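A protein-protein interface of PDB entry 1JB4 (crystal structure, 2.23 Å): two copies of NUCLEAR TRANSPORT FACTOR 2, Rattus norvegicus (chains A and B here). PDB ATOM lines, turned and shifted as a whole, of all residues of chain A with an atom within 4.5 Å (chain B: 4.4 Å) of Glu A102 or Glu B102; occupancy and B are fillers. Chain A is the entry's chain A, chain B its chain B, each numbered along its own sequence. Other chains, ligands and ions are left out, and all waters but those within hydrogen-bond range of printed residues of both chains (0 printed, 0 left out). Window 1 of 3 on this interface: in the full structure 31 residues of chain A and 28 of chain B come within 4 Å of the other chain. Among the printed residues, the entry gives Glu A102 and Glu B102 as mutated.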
ATOM      1  N   ILE A  82      16.245  22.013 -27.823  1.00  0.00           N
ATOM      2  CA  ILE A  82      16.003  23.442 -27.791  1.00  0.00           C
ATOM      3  C   ILE A  82      14.507  23.562 -27.556  1.00  0.00           C
ATOM      4  O   ILE A  82      13.730  22.752 -28.048  1.00  0.00           O
ATOM      5  CB  ILE A  82      16.464  24.147 -29.116  1.00  0.00           C
ATOM      6  CG1 ILE A  82      16.115  25.639 -29.063  1.00  0.00           C
ATOM      7  CG2 ILE A  82      15.867  23.461 -30.335  1.00  0.00           C
ATOM      8  CD1 ILE A  82      16.755  26.454 -30.187  1.00  0.00           C
ATOM      9  N   SER A  83      14.098  24.552 -26.779  1.00  0.00           N
ATOM     10  CA  SER A  83      12.682  24.696 -26.477  1.00  0.00           C
ATOM     11  C   SER A  83      12.201  26.122 -26.558  1.00  0.00           C
ATOM     12  O   SER A  83      12.963  27.067 -26.331  1.00  0.00           O
ATOM     13  CB  SER A  83      12.402  24.173 -25.070  1.00  0.00           C
ATOM     14  OG  SER A  83      13.227  23.057 -24.783  1.00  0.00           O
ATOM     15  N   MET A  84      10.925  26.261 -26.888  1.00  0.00           N
ATOM     16  CA  MET A  84      10.284  27.561 -26.961  1.00  0.00           C
ATOM     17  C   MET A  84       9.057  27.508 -26.047  1.00  0.00           C
ATOM     18  O   MET A  84       8.291  26.546 -26.067  1.00  0.00           O
ATOM     19  CB  MET A  84       9.862  27.892 -28.395  1.00  0.00           C
ATOM     20  CG  MET A  84       9.317  29.313 -28.520  1.00  0.00           C
ATOM     21  SD  MET A  84       9.236  29.958 -30.203  1.00  0.00           S
ATOM     22  CE  MET A  84       8.089  31.294 -29.985  1.00  0.00           C
ATOM     23  N   VAL A  85       8.892  28.532 -25.222  1.00  0.00           N
ATOM     24  CA  VAL A  85       7.763  28.586 -24.309  1.00  0.00           C
ATOM     25  C   VAL A  85       7.094  29.959 -24.346  1.00  0.00           C
ATOM     26  O   VAL A  85       7.768  30.981 -24.243  1.00  0.00           O
ATOM     27  CB  VAL A  85       8.221  28.292 -22.873  1.00  0.00           C
ATOM     28  CG1 VAL A  85       7.139  28.685 -21.896  1.00  0.00           C
ATOM     29  CG2 VAL A  85       8.565  26.818 -22.730  1.00  0.00           C
ATOM     30  N   HIS A 100       7.984  35.154 -23.500  1.00  0.00           N
ATOM     31  CA  HIS A 100       8.601  34.214 -24.406  1.00  0.00           C
ATOM     32  C   HIS A 100       9.881  33.761 -23.695  1.00  0.00           C
ATOM     33  O   HIS A 100      10.672  34.596 -23.231  1.00  0.00           O
ATOM     34  CB  HIS A 100       8.958  34.909 -25.724  1.00  0.00           C
ATOM     35  CG  HIS A 100       9.769  34.064 -26.659  1.00  0.00           C
ATOM     36  ND1 HIS A 100      10.203  34.521 -27.883  1.00  0.00           N
ATOM     37  CD2 HIS A 100      10.241  32.798 -26.544  1.00  0.00           C
ATOM     38  CE1 HIS A 100      10.909  33.576 -28.480  1.00  0.00           C
ATOM     39  NE2 HIS A 100      10.947  32.521 -27.687  1.00  0.00           N
ATOM     40  N   GLN A 101      10.061  32.451 -23.562  1.00  0.00           N
ATOM     41  CA  GLN A 101      11.272  31.925 -22.950  1.00  0.00           C
ATOM     42  C   GLN A 101      11.845  30.835 -23.841  1.00  0.00           C
ATOM     43  O   GLN A 101      11.123  29.999 -24.382  1.00  0.00           O
ATOM     44  CB  GLN A 101      11.018  31.384 -21.543  1.00  0.00           C
ATOM     45  CG  GLN A 101      12.324  31.097 -20.770  1.00  0.00           C
ATOM     46  CD  GLN A 101      12.206  31.375 -19.272  1.00  0.00           C
ATOM     47  OE1 GLN A 101      11.124  31.259 -18.683  1.00  0.00           O
ATOM     48  NE2 GLN A 101      13.323  31.725 -18.648  1.00  0.00           N
ATOM     49  N   GLU A 102      13.164  30.873 -23.979  1.00  0.00           N
ATOM     50  CA  GLU A 102      13.915  29.958 -24.819  1.00  0.00           C
ATOM     51  C   GLU A 102      14.922  29.211 -23.961  1.00  0.00           C
ATOM     52  O   GLU A 102      15.571  29.816 -23.108  1.00  0.00           O
ATOM     53  CB  GLU A 102      14.624  30.789 -25.886  1.00  0.00           C
ATOM     54  CG  GLU A 102      15.426  30.038 -26.899  1.00  0.00           C
ATOM     55  CD  GLU A 102      15.879  30.959 -28.009  1.00  0.00           C
ATOM     56  OE1 GLU A 102      15.188  31.967 -28.262  1.00  0.00           O
ATOM     57  OE2 GLU A 102      16.910  30.683 -28.645  1.00  0.00           O
ATOM     58  N   PHE A 103      15.042  27.905 -24.192  1.00  0.00           N
ATOM     59  CA  PHE A 103      15.967  27.051 -23.446  1.00  0.00           C
ATOM     60  C   PHE A 103      16.740  26.098 -24.369  1.00  0.00           C
ATOM     61  O   PHE A 103      16.212  25.597 -25.372  1.00  0.00           O
ATOM     62  CB  PHE A 103      15.237  26.137 -22.435  1.00  0.00           C
ATOM     63  CG  PHE A 103      14.347  26.851 -21.438  1.00  0.00           C
ATOM     64  CD1 PHE A 103      12.989  27.034 -21.697  1.00  0.00           C
ATOM     65  CD2 PHE A 103      14.854  27.276 -20.211  1.00  0.00           C
ATOM     66  CE1 PHE A 103      12.141  27.628 -20.740  1.00  0.00           C
ATOM     67  CE2 PHE A 103      14.020  27.876 -19.240  1.00  0.00           C
ATOM     68  CZ  PHE A 103      12.661  28.051 -19.503  1.00  0.00           C
ATOM     69  N   ASN A 116      21.563  27.323 -21.731  1.00  0.00           N
ATOM     70  CA  ASN A 116      21.162  28.619 -22.270  1.00  0.00           C
ATOM     71  C   ASN A 116      19.713  28.926 -21.920  1.00  0.00           C
ATOM     72  O   ASN A 116      18.818  28.100 -22.089  1.00  0.00           O
ATOM     73  CB  ASN A 116      21.376  28.627 -23.778  1.00  0.00           C
ATOM     74  CG  ASN A 116      22.839  28.516 -24.145  1.00  0.00           C
ATOM     75  OD1 ASN A 116      23.550  29.529 -24.235  1.00  0.00           O
ATOM     76  ND2 ASN A 116      23.310  27.287 -24.337  1.00  0.00           N
ATOM     77  N   ASP A 117      19.486  30.139 -21.444  1.00  0.00           N
ATOM     78  CA  ASP A 117      18.161  30.535 -21.024  1.00  0.00           C
ATOM     79  C   ASP A 117      17.956  31.984 -21.448  1.00  0.00           C
ATOM     80  O   ASP A 117      18.796  32.834 -21.181  1.00  0.00           O
ATOM     81  CB  ASP A 117      18.102  30.367 -19.496  1.00  0.00           C
ATOM     82  CG  ASP A 117      16.754  30.708 -18.898  1.00  0.00           C
ATOM     83  OD1 ASP A 117      15.904  31.336 -19.576  1.00  0.00           O
ATOM     84  OD2 ASP A 117      16.555  30.351 -17.713  1.00  0.00           O
ATOM     85  N   MET A 118      16.848  32.252 -22.131  1.00  0.00           N
ATOM     86  CA  MET A 118      16.526  33.603 -22.584  1.00  0.00           C
ATOM     87  C   MET A 118      15.031  33.893 -22.341  1.00  0.00           C
ATOM     88  O   MET A 118      14.146  33.165 -22.821  1.00  0.00           O
ATOM     89  CB  MET A 118      16.887  33.771 -24.073  1.00  0.00           C
ATOM     90  CG  MET A 118      18.379  33.604 -24.365  1.00  0.00           C
ATOM     91  SD  MET A 118      18.928  34.052 -26.061  1.00  0.00           S
ATOM     92  CE  MET A 118      18.815  32.444 -26.885  1.00  0.00           C
ATOM     93  N   ILE B  82      23.107  30.372 -29.912  1.00  0.00           N
ATOM     94  CA  ILE B  82      21.652  30.343 -29.827  1.00  0.00           C
ATOM     95  C   ILE B  82      21.128  31.774 -29.814  1.00  0.00           C
ATOM     96  O   ILE B  82      21.680  32.636 -29.126  1.00  0.00           O
ATOM     97  CB  ILE B  82      21.149  29.601 -28.578  1.00  0.00           C
ATOM     98  CG1 ILE B  82      19.624  29.495 -28.662  1.00  0.00           C
ATOM     99  CG2 ILE B  82      21.612  30.311 -27.295  1.00  0.00           C
ATOM    100  CD1 ILE B  82      18.990  28.679 -27.570  1.00  0.00           C
ATOM    101  N   SER B  83      20.050  32.019 -30.552  1.00  0.00           N
ATOM    102  CA  SER B  83      19.501  33.362 -30.660  1.00  0.00           C
ATOM    103  C   SER B  83      18.000  33.482 -30.422  1.00  0.00           C
ATOM    104  O   SER B  83      17.231  32.539 -30.644  1.00  0.00           O
ATOM    105  CB  SER B  83      19.812  33.921 -32.056  1.00  0.00           C
ATOM    106  OG  SER B  83      21.167  33.691 -32.408  1.00  0.00           O
ATOM    107  N   MET B  84      17.594  34.666 -29.977  1.00  0.00           N
ATOM    108  CA  MET B  84      16.188  34.964 -29.764  1.00  0.00           C
ATOM    109  C   MET B  84      15.866  36.257 -30.502  1.00  0.00           C
ATOM    110  O   MET B  84      16.563  37.264 -30.351  1.00  0.00           O
ATOM    111  CB  MET B  84      15.857  35.144 -28.287  1.00  0.00           C
ATOM    112  CG  MET B  84      14.426  35.662 -28.091  1.00  0.00           C
ATOM    113  SD  MET B  84      13.944  35.830 -26.368  1.00  0.00           S
ATOM    114  CE  MET B  84      13.355  34.165 -26.012  1.00  0.00           C
ATOM    115  N   GLN B 101      10.909  34.347 -32.590  1.00  0.00           N
ATOM    116  CA  GLN B 101      11.662  33.320 -33.278  1.00  0.00           C
ATOM    117  C   GLN B 101      12.931  32.970 -32.527  1.00  0.00           C
ATOM    118  O   GLN B 101      13.518  33.803 -31.828  1.00  0.00           O
ATOM    119  CB  GLN B 101      11.968  33.787 -34.708  1.00  0.00           C
ATOM    120  CG  GLN B 101      12.562  32.718 -35.629  1.00  0.00           C
ATOM    121  CD  GLN B 101      12.199  32.922 -37.114  1.00  0.00           C
ATOM    122  OE1 GLN B 101      12.003  34.047 -37.583  1.00  0.00           O
ATOM    123  NE2 GLN B 101      12.125  31.820 -37.851  1.00  0.00           N
ATOM    124  N   GLU B 102      13.317  31.707 -32.646  1.00  0.00           N
ATOM    125  CA  GLU B 102      14.516  31.189 -32.010  1.00  0.00           C
ATOM    126  C   GLU B 102      15.335  30.504 -33.108  1.00  0.00           C
ATOM    127  O   GLU B 102      14.775  29.879 -34.018  1.00  0.00           O
ATOM    128  CB  GLU B 102      14.146  30.177 -30.903  1.00  0.00           C
ATOM    129  CG  GLU B 102      13.192  30.734 -29.830  1.00  0.00           C
ATOM    130  CD  GLU B 102      12.836  29.721 -28.729  1.00  0.00           C
ATOM    131  OE1 GLU B 102      13.449  28.632 -28.674  1.00  0.00           O
ATOM    132  OE2 GLU B 102      11.948  30.021 -27.904  1.00  0.00           O
ATOM    133  N   PHE B 103      16.653  30.662 -33.043  1.00  0.00           N
ATOM    134  CA  PHE B 103      17.540  30.022 -34.005  1.00  0.00           C
ATOM    135  C   PHE B 103      18.683  29.406 -33.232  1.00  0.00           C
ATOM    136  O   PHE B 103      19.087  29.910 -32.186  1.00  0.00           O
ATOM    137  CB  PHE B 103      18.176  31.007 -34.994  1.00  0.00           C
ATOM    138  CG  PHE B 103      17.205  31.837 -35.775  1.00  0.00           C
ATOM    139  CD1 PHE B 103      16.689  33.016 -35.244  1.00  0.00           C
ATOM    140  CD2 PHE B 103      16.871  31.489 -37.082  1.00  0.00           C
ATOM    141  CE1 PHE B 103      15.863  33.843 -36.009  1.00  0.00           C
ATOM    142  CE2 PHE B 103      16.041  32.314 -37.859  1.00  0.00           C
ATOM    143  CZ  PHE B 103      15.540  33.489 -37.328  1.00  0.00           C
ATOM    144  N   ASN B 116      18.280  24.604 -36.006  1.00  0.00           N
ATOM    145  CA  ASN B 116      17.008  24.684 -35.318  1.00  0.00           C
ATOM    146  C   ASN B 116      16.377  26.049 -35.459  1.00  0.00           C
ATOM    147  O   ASN B 116      16.995  27.072 -35.152  1.00  0.00           O
ATOM    148  CB  ASN B 116      17.220  24.328 -33.845  1.00  0.00           C
ATOM    149  CG  ASN B 116      17.720  22.899 -33.662  1.00  0.00           C
ATOM    150  OD1 ASN B 116      16.930  21.963 -33.551  1.00  0.00           O
ATOM    151  ND2 ASN B 116      19.038  22.726 -33.656  1.00  0.00           N
ATOM    152  N   ASP B 117      15.134  26.052 -35.930  1.00  0.00           N
ATOM    153  CA  ASP B 117      14.374  27.274 -36.163  1.00  0.00           C
ATOM    154  C   ASP B 117      12.997  27.094 -35.530  1.00  0.00           C
ATOM    155  O   ASP B 117      12.315  26.101 -35.783  1.00  0.00           O
ATOM    156  CB  ASP B 117      14.229  27.483 -37.673  1.00  0.00           C
ATOM    157  CG  ASP B 117      13.597  28.822 -38.041  1.00  0.00           C
ATOM    158  OD1 ASP B 117      12.898  29.427 -37.194  1.00  0.00           O
ATOM    159  OD2 ASP B 117      13.792  29.259 -39.202  1.00  0.00           O
ATOM    160  N   MET B 118      12.592  28.046 -34.700  1.00  0.00           N
ATOM    161  CA  MET B 118      11.281  27.974 -34.051  1.00  0.00           C
ATOM    162  C   MET B 118      10.597  29.332 -34.190  1.00  0.00           C
ATOM    163  O   MET B 118      11.172  30.359 -33.830  1.00  0.00           O
ATOM    164  CB  MET B 118      11.434  27.534 -32.580  1.00  0.00           C
ATOM    165  CG  MET B 118      12.039  26.129 -32.439  1.00  0.00           C
ATOM    166  SD  MET B 118      12.123  25.396 -30.748  1.00  0.00           S
ATOM    167  CE  MET B 118      10.535  24.652 -30.612  1.00  0.00           C
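Ile A82 touches Asn B116. Met A84 touches Met B118 (CB to CE, 3.98 Å). NE2 of His A100 touches CE of Met B84, at 3.4 Å. Ile B82 touches Glu A102. Met B84 touches Glu A102 (CB to OE1, 3.2 Å). Glu A102 touches Glu B102. CG2 of Ile B82 touches OD1 of Asn A116, 3.7 Å away. Met A118 touches Ile B82 (CE to CG1, 3.5 Å). Ser B83 touches Met A118. O of Met A118 touches CE of Met B84, at 3.4 Å.
Ile A82 touches Asn B116, and with the chains exchanged Asn A116 touches Ile B82. Ser A83 touches Glu B102, and with the chains exchanged Glu A102 touches Ser B83. Met A84 touches Met B118, and with the chains exchanged Met A118 touches Met B84. Met A118 touches Ile B82, but with the chains exchanged Ile A82 does not touch Met B118 (4.1 Å).
Printed residues of chain B within 4 Å of Glu A102: Ile B82, Ser B83, Met B84 and Glu B102. Glu B102 touches just these residues of chain A: Ser A83 (2.9 Å), Met A84 (2.8 Å), His A100 (2.7 Å), Gln A101 (3.6 Å) and Glu A102 (2.8 Å). Of the printed residues of chain B, Ile A82 touches Asn B116. Of the printed residues of chain B, Met A84 touches Glu B102 and Met B118. Of the printed residues of chain B, Met A118 touches Ile B82 (3.5 Å), Ser B83 (3.8 Å) and Met B84 (3.4 Å). Of the printed residues of chain B, His A100 touches Met B84 and Glu B102. Of the printed residues of chain A, Ile B82 touches Glu A102, Asn A116 and Met A118. The nearest printed residue of chain B that does not touch His A100 is Gln B101 (4.2 Å).
The side-chain carboxylate (OE1) of Glu B102 sits close to the backbone carbonyl oxygen (O) of Ser A83. The side-chain carboxylate of Glu A102 lies close to the backbone carbonyl oxygen of Ser B83, 2.7 Å away. NE2 of His A100 sits at hydrogen-bond distance from OE2 of Glu B102 (2.7 Å). The side-chain sulfur (SD) of Met A84 sits close to the side-chain carboxylate (OE2) of Glu B102, at 3.6 Å.
Of the 11 printed residues of chain A, 8 touch a printed residue of chain B. Printed residues of chain A that touch a printed residue of chain B: Ile A82, Ser A83, Met A84, His A100, Gln A101, Glu A102, Asn A116 and Met A118. Of the 9 printed residues of chain B, 6 touch a printed residue of chain A. Printed residues of chain B that touch a printed residue of chain A: Ile B82, Ser B83, Met B84, Glu B102, Asn B116 and Met B118. Hydrophobic or aromatic side chains of chain B that line the printed part of chain A: Ile B82, Met B84 and Met B118. Among the printed residues, no Asp or Glu carboxylate lies within 4 Å of a Lys or Arg side-chain nitrogen of the other chain.
N of Glu B102 sits at hydrogen-bond distance from O of Met B118, at 2.8 Å. N of Glu A102 is in hydrogen-bond range of O of Met A118, at 2.7 Å. O of Phe A103 lies within hydrogen-bond range of N of Ser A83 (2.7 Å). OD1 of Asp A117 sits at hydrogen-bond distance from NE2 of Gln A101, at 2.8 Å. The backbone NH (N) of Ser B83 lies within hydrogen-bond range of the backbone carbonyl oxygen (O) of Phe B103, at 2.8 Å. N of Val A85 sits at hydrogen-bond distance from O of Gln A101 (2.8 Å).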
